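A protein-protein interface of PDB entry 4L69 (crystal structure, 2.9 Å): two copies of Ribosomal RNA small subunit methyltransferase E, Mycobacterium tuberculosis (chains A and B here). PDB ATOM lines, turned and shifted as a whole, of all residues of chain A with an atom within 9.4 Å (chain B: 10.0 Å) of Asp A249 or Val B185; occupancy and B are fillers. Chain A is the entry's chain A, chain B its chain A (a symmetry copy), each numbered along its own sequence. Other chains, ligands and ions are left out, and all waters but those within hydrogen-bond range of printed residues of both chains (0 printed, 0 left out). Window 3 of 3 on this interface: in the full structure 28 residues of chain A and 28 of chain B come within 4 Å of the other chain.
O of Pro A78 sits close to NH1 of Arg A247. The backbone NH of Trp A248 sits close to the backbone carbonyl oxygen of Gly A242, 3.4 Å away. The side-chain hydroxyl of Thr A245 lies close to the backbone NH of Arg A247, at 3.5 Å. The backbone carbonyl oxygen (O) of Arg B222 sits at hydrogen-bond distance from the backbone NH (N) of Ile B184. The backbone carbonyl oxygen (O) of Gly B224 is in hydrogen-bond range of the guanidinium group (NE) of Arg B222 (3.0 Å).
Ala A240 touches Val B243. Leu B244 touches Val A243 (CD2 to CG1, 3.7 Å). Val B243 touches Leu A244. Arg A247 touches Pro B225. CZ3 of Trp A248 touches CG2 of Ile B184, at 3.7 Å. Leu B223 touches Trp A248 (CD2 to CZ3, 3.6 Å). Gly B224 touches Trp A248. CD of Pro B225 touches CD1 of Trp A248, at 3.9 Å. CZ3 of Trp A248 touches CB of Ala B240 (3.8 Å). Val B185 touches Asp A249.
Val A243 touches just these residues of chain B: Ala B240 (3.6 Å), Val B243 (3.8 Å) and Leu B244 (3.7 Å). Asp A249 touches one residue of chain B. Val B185 touches one residue of chain A. No residue of chain A comes within 4 Å of Asp B186. Of the printed residues of chain A, Pro B225 touches Arg A247 (3.7 Å) and Trp A248 (3.9 Å). Ala B237 touches none of the printed residues of chain A. Of the printed residues of chain A, Leu B244 touches Val A243 (3.7 Å).
Of the 25 printed residues of chain B, 8 touch a printed residue of chain A. Hydrophobic or aromatic side chains of chain B within 4 Å of the printed part of chain A: Ile B184, Val B185, Leu B223, Pro B225, Ala B240, Val B243 and Leu B244. Among the printed residues, 13 pairs touch across the chains. Among the printed residues, no Asp or Glu carboxylate lies within 4 Å of a Lys or Arg side-chain nitrogen of the other chain.
Ala A240 touches Val B243, and with the chains exchanged Val A243 touches Ala B240. Val B243 touches its own counterpart, Val A243. Val A243 touches Leu B244, and with the chains exchanged Leu A244 touches Val B243. Positions printed for both chains: 190, 240, 241, 243, 244 and 245.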
ATOM      1  N   VAL A  76     -14.709  -6.522 -21.745  1.00  0.00           N
ATOM      2  CA  VAL A  76     -14.707  -7.679 -22.650  1.00  0.00           C
ATOM      3  C   VAL A  76     -14.948  -7.209 -24.073  1.00  0.00           C
ATOM      4  O   VAL A  76     -15.951  -6.537 -24.318  1.00  0.00           O
ATOM      5  CB  VAL A  76     -15.742  -8.762 -22.212  1.00  0.00           C
ATOM      6  CG1 VAL A  76     -15.790  -9.932 -23.201  1.00  0.00           C
ATOM      7  CG2 VAL A  76     -15.457  -9.265 -20.797  1.00  0.00           C
ATOM      8  N   ARG A  77     -14.039  -7.556 -25.001  1.00  0.00           N
ATOM      9  CA  ARG A  77     -14.169  -7.200 -26.416  1.00  0.00           C
ATOM     10  C   ARG A  77     -14.140  -8.443 -27.340  1.00  0.00           C
ATOM     11  O   ARG A  77     -13.324  -9.331 -27.119  1.00  0.00           O
ATOM     12  CB  ARG A  77     -13.152  -6.123 -26.844  1.00  0.00           C
ATOM     13  N   PRO A  78     -15.029  -8.558 -28.355  1.00  0.00           N
ATOM     14  CA  PRO A  78     -16.095  -7.612 -28.732  1.00  0.00           C
ATOM     15  C   PRO A  78     -17.245  -7.578 -27.716  1.00  0.00           C
ATOM     16  O   PRO A  78     -17.742  -8.634 -27.303  1.00  0.00           O
ATOM     17  CB  PRO A  78     -16.543  -8.124 -30.107  1.00  0.00           C
ATOM     18  CG  PRO A  78     -16.283  -9.594 -30.054  1.00  0.00           C
ATOM     19  CD  PRO A  78     -15.021  -9.740 -29.240  1.00  0.00           C
ATOM     20  N   ALA A 190     -16.056 -13.116 -36.099  1.00  0.00           N
ATOM     21  CA  ALA A 190     -14.693 -12.908 -35.588  1.00  0.00           C
ATOM     22  C   ALA A 190     -14.017 -11.589 -36.020  1.00  0.00           C
ATOM     23  O   ALA A 190     -13.178 -11.062 -35.280  1.00  0.00           O
ATOM     24  CB  ALA A 190     -13.815 -14.102 -35.920  1.00  0.00           C
ATOM     25  N   GLY A 239     -23.975 -17.784 -26.031  1.00  0.00           N
ATOM     26  CA  GLY A 239     -23.179 -19.003 -26.009  1.00  0.00           C
ATOM     27  C   GLY A 239     -22.634 -19.330 -27.383  1.00  0.00           C
ATOM     28  O   GLY A 239     -21.522 -19.841 -27.511  1.00  0.00           O
ATOM     29  N   ALA A 240     -23.410 -19.022 -28.423  1.00  0.00           N
ATOM     30  CA  ALA A 240     -23.014 -19.217 -29.810  1.00  0.00           C
ATOM     31  C   ALA A 240     -21.961 -18.157 -30.172  1.00  0.00           C
ATOM     32  O   ALA A 240     -20.882 -18.504 -30.663  1.00  0.00           O
ATOM     33  CB  ALA A 240     -24.228 -19.093 -30.716  1.00  0.00           C
ATOM     34  N   VAL A 241     -22.260 -16.874 -29.859  1.00  0.00           N
ATOM     35  CA  VAL A 241     -21.392 -15.708 -30.080  1.00  0.00           C
ATOM     36  C   VAL A 241     -20.032 -15.862 -29.352  1.00  0.00           C
ATOM     37  O   VAL A 241     -19.008 -15.484 -29.901  1.00  0.00           O
ATOM     38  CB  VAL A 241     -22.142 -14.380 -29.758  1.00  0.00           C
ATOM     39  CG1 VAL A 241     -21.190 -13.208 -29.553  1.00  0.00           C
ATOM     40  CG2 VAL A 241     -23.179 -14.055 -30.832  1.00  0.00           C
ATOM     41  N   GLY A 242     -20.030 -16.461 -28.165  1.00  0.00           N
ATOM     42  CA  GLY A 242     -18.810 -16.696 -27.401  1.00  0.00           C
ATOM     43  C   GLY A 242     -17.835 -17.599 -28.126  1.00  0.00           C
ATOM     44  O   GLY A 242     -16.627 -17.360 -28.113  1.00  0.00           O
ATOM     45  N   VAL A 243     -18.360 -18.624 -28.788  1.00  0.00           N
ATOM     46  CA  VAL A 243     -17.572 -19.575 -29.554  1.00  0.00           C
ATOM     47  C   VAL A 243     -17.115 -18.971 -30.915  1.00  0.00           C
ATOM     48  O   VAL A 243     -15.938 -19.085 -31.268  1.00  0.00           O
ATOM     49  CB  VAL A 243     -18.347 -20.911 -29.663  1.00  0.00           C
ATOM     50  CG1 VAL A 243     -17.855 -21.774 -30.821  1.00  0.00           C
ATOM     51  CG2 VAL A 243     -18.260 -21.675 -28.348  1.00  0.00           C
ATOM     52  N   LEU A 244     -18.034 -18.309 -31.644  1.00  0.00           N
ATOM     53  CA  LEU A 244     -17.771 -17.678 -32.943  1.00  0.00           C
ATOM     54  C   LEU A 244     -16.779 -16.519 -32.856  1.00  0.00           C
ATOM     55  O   LEU A 244     -16.035 -16.292 -33.809  1.00  0.00           O
ATOM     56  CB  LEU A 244     -19.076 -17.189 -33.606  1.00  0.00           C
ATOM     57  CG  LEU A 244     -20.098 -18.254 -33.984  1.00  0.00           C
ATOM     58  CD1 LEU A 244     -21.500 -17.690 -33.964  1.00  0.00           C
ATOM     59  CD2 LEU A 244     -19.785 -18.864 -35.318  1.00  0.00           C
ATOM     60  N   THR A 245     -16.776 -15.786 -31.736  1.00  0.00           N
ATOM     61  CA  THR A 245     -15.897 -14.638 -31.518  1.00  0.00           C
ATOM     62  C   THR A 245     -14.766 -14.963 -30.533  1.00  0.00           C
ATOM     63  O   THR A 245     -14.725 -16.056 -29.964  1.00  0.00           O
ATOM     64  CB  THR A 245     -16.710 -13.391 -31.090  1.00  0.00           C
ATOM     65  OG1 THR A 245     -17.226 -13.579 -29.771  1.00  0.00           O
ATOM     66  CG2 THR A 245     -17.839 -13.054 -32.051  1.00  0.00           C
ATOM     67  N   SER A 246     -13.854 -13.997 -30.330  1.00  0.00           N
ATOM     68  CA  SER A 246     -12.699 -14.075 -29.420  1.00  0.00           C
ATOM     69  C   SER A 246     -13.102 -13.887 -27.940  1.00  0.00           C
ATOM     70  O   SER A 246     -12.239 -13.889 -27.053  1.00  0.00           O
ATOM     71  CB  SER A 246     -11.637 -13.056 -29.827  1.00  0.00           C
ATOM     72  OG  SER A 246     -12.199 -11.902 -30.436  1.00  0.00           O
ATOM     73  N   ARG A 247     -14.421 -13.750 -27.686  1.00  0.00           N
ATOM     74  CA  ARG A 247     -15.029 -13.563 -26.372  1.00  0.00           C
ATOM     75  C   ARG A 247     -14.698 -14.675 -25.365  1.00  0.00           C
ATOM     76  O   ARG A 247     -14.597 -14.402 -24.170  1.00  0.00           O
ATOM     77  CB  ARG A 247     -16.536 -13.408 -26.527  1.00  0.00           C
ATOM     78  CG  ARG A 247     -16.951 -11.975 -26.797  1.00  0.00           C
ATOM     79  CD  ARG A 247     -18.426 -11.867 -27.117  1.00  0.00           C
ATOM     80  NE  ARG A 247     -19.280 -12.375 -26.042  1.00  0.00           N
ATOM     81  CZ  ARG A 247     -19.767 -11.633 -25.054  1.00  0.00           C
ATOM     82  NH1 ARG A 247     -19.490 -10.337 -24.988  1.00  0.00           N
ATOM     83  NH2 ARG A 247     -20.540 -12.181 -24.124  1.00  0.00           N
ATOM     84  N   TRP A 248     -14.537 -15.916 -25.845  1.00  0.00           N
ATOM     85  CA  TRP A 248     -14.205 -17.077 -25.022  1.00  0.00           C
ATOM     86  C   TRP A 248     -12.817 -17.618 -25.411  1.00  0.00           C
ATOM     87  O   TRP A 248     -12.163 -18.281 -24.597  1.00  0.00           O
ATOM     88  CB  TRP A 248     -15.270 -18.180 -25.188  1.00  0.00           C
ATOM     89  CG  TRP A 248     -16.615 -17.906 -24.568  1.00  0.00           C
ATOM     90  CD1 TRP A 248     -17.039 -16.751 -23.977  1.00  0.00           C
ATOM     91  CD2 TRP A 248     -17.714 -18.826 -24.480  1.00  0.00           C
ATOM     92  NE1 TRP A 248     -18.322 -16.902 -23.502  1.00  0.00           N
ATOM     93  CE2 TRP A 248     -18.766 -18.161 -23.812  1.00  0.00           C
ATOM     94  CE3 TRP A 248     -17.910 -20.154 -24.894  1.00  0.00           C
ATOM     95  CZ2 TRP A 248     -20.000 -18.772 -23.567  1.00  0.00           C
ATOM     96  CZ3 TRP A 248     -19.130 -20.757 -24.646  1.00  0.00           C
ATOM     97  CH2 TRP A 248     -20.156 -20.073 -23.986  1.00  0.00           C
ATOM     98  N   ASP A 249     -12.377 -17.329 -26.655  1.00  0.00           N
ATOM     99  CA  ASP A 249     -11.101 -17.772 -27.235  1.00  0.00           C
ATOM    100  C   ASP A 249      -9.894 -17.071 -26.593  1.00  0.00           C
ATOM    101  O   ASP A 249      -9.554 -17.343 -25.437  1.00  0.00           O
ATOM    102  CB  ASP A 249     -11.109 -17.576 -28.771  1.00  0.00           C
ATOM    103  CG  ASP A 249     -12.259 -18.255 -29.529  1.00  0.00           C
ATOM    104  OD1 ASP A 249     -13.380 -18.356 -28.962  1.00  0.00           O
ATOM    105  OD2 ASP A 249     -12.053 -18.635 -30.707  1.00  0.00           O
ATOM    106  N   LEU B 174     -18.810 -33.653 -21.529  1.00  0.00           N
ATOM    107  CA  LEU B 174     -18.244 -32.380 -21.080  1.00  0.00           C
ATOM    108  C   LEU B 174     -18.770 -32.011 -19.705  1.00  0.00           C
ATOM    109  O   LEU B 174     -19.987 -31.952 -19.507  1.00  0.00           O
ATOM    110  CB  LEU B 174     -18.537 -31.254 -22.104  1.00  0.00           C
ATOM    111  CG  LEU B 174     -18.120 -31.513 -23.565  1.00  0.00           C
ATOM    112  CD1 LEU B 174     -18.911 -30.651 -24.517  1.00  0.00           C
ATOM    113  CD2 LEU B 174     -16.639 -31.282 -23.766  1.00  0.00           C
ATOM    114  N   LEU B 176     -19.118 -29.137 -17.162  1.00  0.00           N
ATOM    115  CA  LEU B 176     -19.024 -27.680 -17.078  1.00  0.00           C
ATOM    116  C   LEU B 176     -18.459 -27.290 -15.713  1.00  0.00           C
ATOM    117  O   LEU B 176     -19.168 -27.315 -14.702  1.00  0.00           O
ATOM    118  CB  LEU B 176     -20.350 -26.957 -17.397  1.00  0.00           C
ATOM    119  CG  LEU B 176     -21.086 -27.357 -18.672  1.00  0.00           C
ATOM    120  CD1 LEU B 176     -22.382 -26.609 -18.788  1.00  0.00           C
ATOM    121  CD2 LEU B 176     -20.236 -27.146 -19.923  1.00  0.00           C
ATOM    122  N   THR B 181      -9.009 -26.176 -16.994  1.00  0.00           N
ATOM    123  CA  THR B 181      -7.885 -25.673 -17.791  1.00  0.00           C
ATOM    124  C   THR B 181      -8.162 -25.789 -19.303  1.00  0.00           C
ATOM    125  O   THR B 181      -7.392 -25.257 -20.111  1.00  0.00           O
ATOM    126  CB  THR B 181      -6.541 -26.304 -17.352  1.00  0.00           C
ATOM    127  OG1 THR B 181      -6.541 -27.707 -17.627  1.00  0.00           O
ATOM    128  CG2 THR B 181      -6.217 -26.049 -15.885  1.00  0.00           C
ATOM    129  N   GLU B 182      -9.270 -26.473 -19.677  1.00  0.00           N
ATOM    130  CA  GLU B 182      -9.669 -26.691 -21.066  1.00  0.00           C
ATOM    131  C   GLU B 182     -10.911 -25.890 -21.416  1.00  0.00           C
ATOM    132  O   GLU B 182     -11.822 -25.775 -20.594  1.00  0.00           O
ATOM    133  CB  GLU B 182      -9.900 -28.183 -21.326  1.00  0.00           C
ATOM    134  CG  GLU B 182      -9.520 -28.617 -22.730  1.00  0.00           C
ATOM    135  CD  GLU B 182      -8.370 -29.602 -22.792  1.00  0.00           C
ATOM    136  OE1 GLU B 182      -8.528 -30.739 -22.288  1.00  0.00           O
ATOM    137  OE2 GLU B 182      -7.314 -29.241 -23.358  1.00  0.00           O
ATOM    138  N   ARG B 183     -10.946 -25.345 -22.644  1.00  0.00           N
ATOM    139  CA  ARG B 183     -12.053 -24.538 -23.166  1.00  0.00           C
ATOM    140  C   ARG B 183     -12.945 -25.354 -24.089  1.00  0.00           C
ATOM    141  O   ARG B 183     -12.441 -26.218 -24.815  1.00  0.00           O
ATOM    142  CB  ARG B 183     -11.514 -23.317 -23.924  1.00  0.00           C
ATOM    143  N   ILE B 184     -14.270 -25.059 -24.077  1.00  0.00           N
ATOM    144  CA  ILE B 184     -15.290 -25.708 -24.914  1.00  0.00           C
ATOM    145  C   ILE B 184     -14.973 -25.565 -26.411  1.00  0.00           C
ATOM    146  O   ILE B 184     -15.192 -26.508 -27.174  1.00  0.00           O
ATOM    147  CB  ILE B 184     -16.736 -25.258 -24.531  1.00  0.00           C
ATOM    148  CG1 ILE B 184     -17.819 -26.150 -25.177  1.00  0.00           C
ATOM    149  CG2 ILE B 184     -16.988 -23.766 -24.781  1.00  0.00           C
ATOM    150  CD1 ILE B 184     -19.000 -26.429 -24.317  1.00  0.00           C
ATOM    151  N   VAL B 185     -14.418 -24.395 -26.804  1.00  0.00           N
ATOM    152  CA  VAL B 185     -14.009 -24.013 -28.165  1.00  0.00           C
ATOM    153  C   VAL B 185     -13.075 -25.074 -28.759  1.00  0.00           C
ATOM    154  O   VAL B 185     -13.375 -25.635 -29.817  1.00  0.00           O
ATOM    155  CB  VAL B 185     -13.354 -22.596 -28.214  1.00  0.00           C
ATOM    156  CG1 VAL B 185     -13.542 -21.954 -29.588  1.00  0.00           C
ATOM    157  CG2 VAL B 185     -13.881 -21.677 -27.110  1.00  0.00           C
ATOM    158  N   ASP B 186     -11.966 -25.365 -28.054  1.00  0.00           N
ATOM    159  CA  ASP B 186     -10.981 -26.360 -28.468  1.00  0.00           C
ATOM    160  C   ASP B 186     -11.325 -27.769 -27.956  1.00  0.00           C
ATOM    161  O   ASP B 186     -10.637 -28.318 -27.092  1.00  0.00           O
ATOM    162  CB  ASP B 186      -9.529 -25.921 -28.152  1.00  0.00           C
ATOM    163  CG  ASP B 186      -9.307 -25.254 -26.804  1.00  0.00           C
ATOM    164  OD1 ASP B 186      -9.385 -25.959 -25.771  1.00  0.00           O
ATOM    165  OD2 ASP B 186      -8.987 -24.043 -26.786  1.00  0.00           O
ATOM    166  N   ILE B 187     -12.413 -28.339 -28.493  1.00  0.00           N
ATOM    167  CA  ILE B 187     -12.872 -29.686 -28.159  1.00  0.00           C
ATOM    168  C   ILE B 187     -13.280 -30.446 -29.427  1.00  0.00           C
ATOM    169  O   ILE B 187     -13.805 -29.830 -30.365  1.00  0.00           O
ATOM    170  CB  ILE B 187     -13.921 -29.701 -26.993  1.00  0.00           C
ATOM    171  CG1 ILE B 187     -13.554 -30.742 -25.915  1.00  0.00           C
ATOM    172  CG2 ILE B 187     -15.387 -29.826 -27.451  1.00  0.00           C
ATOM    173  CD1 ILE B 187     -12.447 -30.304 -24.918  1.00  0.00           C
ATOM    174  N   ALA B 188     -13.023 -31.772 -29.463  1.00  0.00           N
ATOM    175  CA  ALA B 188     -13.324 -32.649 -30.605  1.00  0.00           C
ATOM    176  C   ALA B 188     -14.847 -32.863 -30.833  1.00  0.00           C
ATOM    177  O   ALA B 188     -15.290 -33.980 -31.124  1.00  0.00           O
ATOM    178  CB  ALA B 188     -12.602 -33.981 -30.432  1.00  0.00           C
ATOM    179  N   ALA B 189     -15.626 -31.762 -30.751  1.00  0.00           N
ATOM    180  CA  ALA B 189     -17.087 -31.700 -30.856  1.00  0.00           C
ATOM    181  C   ALA B 189     -17.734 -32.216 -32.152  1.00  0.00           C
ATOM    182  O   ALA B 189     -18.689 -33.000 -32.069  1.00  0.00           O
ATOM    183  CB  ALA B 189     -17.577 -30.292 -30.536  1.00  0.00           C
ATOM    184  N   ALA B 190     -17.252 -31.763 -33.335  1.00  0.00           N
ATOM    185  CA  ALA B 190     -17.821 -32.139 -34.638  1.00  0.00           C
ATOM    186  C   ALA B 190     -17.684 -33.630 -35.014  1.00  0.00           C
ATOM    187  O   ALA B 190     -18.533 -34.156 -35.745  1.00  0.00           O
ATOM    188  CB  ALA B 190     -17.263 -31.250 -35.735  1.00  0.00           C
ATOM    189  N   VAL B 219     -14.428 -34.659 -19.831  1.00  0.00           N
ATOM    190  CA  VAL B 219     -13.430 -33.591 -19.888  1.00  0.00           C
ATOM    191  C   VAL B 219     -14.030 -32.353 -19.239  1.00  0.00           C
ATOM    192  O   VAL B 219     -15.137 -31.953 -19.614  1.00  0.00           O
ATOM    193  CB  VAL B 219     -12.938 -33.296 -21.330  1.00  0.00           C
ATOM    194  CG1 VAL B 219     -11.851 -32.223 -21.336  1.00  0.00           C
ATOM    195  CG2 VAL B 219     -12.448 -34.560 -22.021  1.00  0.00           C
ATOM    196  N   ALA B 220     -13.313 -31.758 -18.262  1.00  0.00           N
ATOM    197  CA  ALA B 220     -13.759 -30.533 -17.601  1.00  0.00           C
ATOM    198  C   ALA B 220     -13.537 -29.404 -18.588  1.00  0.00           C
ATOM    199  O   ALA B 220     -12.442 -29.241 -19.125  1.00  0.00           O
ATOM    200  CB  ALA B 220     -12.994 -30.291 -16.311  1.00  0.00           C
ATOM    201  N   VAL B 221     -14.612 -28.698 -18.901  1.00  0.00           N
ATOM    202  CA  VAL B 221     -14.627 -27.631 -19.884  1.00  0.00           C
ATOM    203  C   VAL B 221     -15.233 -26.360 -19.264  1.00  0.00           C
ATOM    204  O   VAL B 221     -16.107 -26.446 -18.391  1.00  0.00           O
ATOM    205  CB  VAL B 221     -15.322 -28.162 -21.172  1.00  0.00           C
ATOM    206  CG1 VAL B 221     -16.572 -27.379 -21.556  1.00  0.00           C
ATOM    207  CG2 VAL B 221     -14.344 -28.259 -22.330  1.00  0.00           C
ATOM    208  N   ARG B 222     -14.723 -25.193 -19.684  1.00  0.00           N
ATOM    209  CA  ARG B 222     -15.134 -23.875 -19.198  1.00  0.00           C
ATOM    210  C   ARG B 222     -15.973 -23.140 -20.257  1.00  0.00           C
ATOM    211  O   ARG B 222     -15.767 -23.343 -21.455  1.00  0.00           O
ATOM    212  CB  ARG B 222     -13.871 -23.064 -18.844  1.00  0.00           C
ATOM    213  CG  ARG B 222     -14.104 -21.832 -17.978  1.00  0.00           C
ATOM    214  CD  ARG B 222     -12.784 -21.202 -17.591  1.00  0.00           C
ATOM    215  NE  ARG B 222     -12.775 -19.759 -17.823  1.00  0.00           N
ATOM    216  CZ  ARG B 222     -11.772 -19.101 -18.399  1.00  0.00           C
ATOM    217  NH1 ARG B 222     -10.687 -19.750 -18.806  1.00  0.00           N
ATOM    218  NH2 ARG B 222     -11.845 -17.788 -18.570  1.00  0.00           N
ATOM    219  N   LEU B 223     -16.908 -22.283 -19.815  1.00  0.00           N
ATOM    220  CA  LEU B 223     -17.734 -21.491 -20.730  1.00  0.00           C
ATOM    221  C   LEU B 223     -17.323 -20.029 -20.650  1.00  0.00           C
ATOM    222  O   LEU B 223     -18.083 -19.184 -20.177  1.00  0.00           O
ATOM    223  CB  LEU B 223     -19.242 -21.644 -20.445  1.00  0.00           C
ATOM    224  CG  LEU B 223     -19.907 -22.979 -20.730  1.00  0.00           C
ATOM    225  CD1 LEU B 223     -21.359 -22.929 -20.319  1.00  0.00           C
ATOM    226  CD2 LEU B 223     -19.829 -23.343 -22.199  1.00  0.00           C
ATOM    227  N   GLY B 224     -16.110 -19.746 -21.097  1.00  0.00           N
ATOM    228  CA  GLY B 224     -15.563 -18.397 -21.097  1.00  0.00           C
ATOM    229  C   GLY B 224     -15.420 -17.775 -19.717  1.00  0.00           C
ATOM    230  O   GLY B 224     -15.391 -18.499 -18.711  1.00  0.00           O
ATOM    231  N   PRO B 225     -15.343 -16.417 -19.637  1.00  0.00           N
ATOM    232  CA  PRO B 225     -15.185 -15.765 -18.323  1.00  0.00           C
ATOM    233  C   PRO B 225     -16.441 -15.823 -17.460  1.00  0.00           C
ATOM    234  O   PRO B 225     -16.370 -15.583 -16.253  1.00  0.00           O
ATOM    235  CB  PRO B 225     -14.800 -14.316 -18.674  1.00  0.00           C
ATOM    236  CG  PRO B 225     -14.591 -14.283 -20.157  1.00  0.00           C
ATOM    237  CD  PRO B 225     -15.377 -15.417 -20.722  1.00  0.00           C
ATOM    238  N   ALA B 237     -24.321 -23.489 -22.841  1.00  0.00           N
ATOM    239  CA  ALA B 237     -23.475 -24.547 -23.396  1.00  0.00           C
ATOM    240  C   ALA B 237     -24.117 -25.149 -24.624  1.00  0.00           C
ATOM    241  O   ALA B 237     -23.402 -25.448 -25.577  1.00  0.00           O
ATOM    242  CB  ALA B 237     -23.203 -25.623 -22.360  1.00  0.00           C
ATOM    243  N   ALA B 240     -23.395 -22.998 -27.563  1.00  0.00           N
ATOM    244  CA  ALA B 240     -22.006 -23.180 -27.955  1.00  0.00           C
ATOM    245  C   ALA B 240     -21.892 -24.488 -28.757  1.00  0.00           C
ATOM    246  O   ALA B 240     -21.360 -24.483 -29.871  1.00  0.00           O
ATOM    247  CB  ALA B 240     -21.123 -23.234 -26.719  1.00  0.00           C
ATOM    248  N   VAL B 241     -22.459 -25.588 -28.206  1.00  0.00           N
ATOM    249  CA  VAL B 241     -22.502 -26.928 -28.807  1.00  0.00           C
ATOM    250  C   VAL B 241     -23.206 -26.913 -30.188  1.00  0.00           C
ATOM    251  O   VAL B 241     -22.766 -27.601 -31.097  1.00  0.00           O
ATOM    252  CB  VAL B 241     -23.079 -27.975 -27.807  1.00  0.00           C
ATOM    253  CG1 VAL B 241     -23.540 -29.252 -28.501  1.00  0.00           C
ATOM    254  CG2 VAL B 241     -22.077 -28.293 -26.698  1.00  0.00           C
ATOM    255  N   VAL B 243     -23.214 -24.504 -32.410  1.00  0.00           N
ATOM    256  CA  VAL B 243     -22.282 -23.917 -33.358  1.00  0.00           C
ATOM    257  C   VAL B 243     -21.085 -24.871 -33.645  1.00  0.00           C
ATOM    258  O   VAL B 243     -20.738 -25.081 -34.811  1.00  0.00           O
ATOM    259  CB  VAL B 243     -21.884 -22.501 -32.875  1.00  0.00           C
ATOM    260  CG1 VAL B 243     -20.580 -22.019 -33.504  1.00  0.00           C
ATOM    261  CG2 VAL B 243     -23.012 -21.517 -33.151  1.00  0.00           C
ATOM    262  N   LEU B 244     -20.493 -25.464 -32.590  1.00  0.00           N
ATOM    263  CA  LEU B 244     -19.359 -26.391 -32.683  1.00  0.00           C
ATOM    264  C   LEU B 244     -19.703 -27.687 -33.415  1.00  0.00           C
ATOM    265  O   LEU B 244     -18.832 -28.257 -34.071  1.00  0.00           O
ATOM    266  CB  LEU B 244     -18.788 -26.725 -31.289  1.00  0.00           C
ATOM    267  CG  LEU B 244     -18.178 -25.573 -30.501  1.00  0.00           C
ATOM    268  CD1 LEU B 244     -18.289 -25.816 -29.013  1.00  0.00           C
ATOM    269  CD2 LEU B 244     -16.752 -25.331 -30.899  1.00  0.00           C
ATOM    270  N   THR B 245     -20.951 -28.157 -33.296  1.00  0.00           N
ATOM    271  CA  THR B 245     -21.419 -29.392 -33.923  1.00  0.00           C
ATOM    272  C   THR B 245     -22.336 -29.112 -35.122  1.00  0.00           C
ATOM    273  O   THR B 245     -22.665 -27.958 -35.403  1.00  0.00           O
ATOM    274  CB  THR B 245     -22.082 -30.326 -32.881  1.00  0.00           C
ATOM    275  OG1 THR B 245     -23.323 -29.765 -32.448  1.00  0.00           O
ATOM    276  CG2 THR B 245     -21.191 -30.613 -31.682  1.00  0.00           C
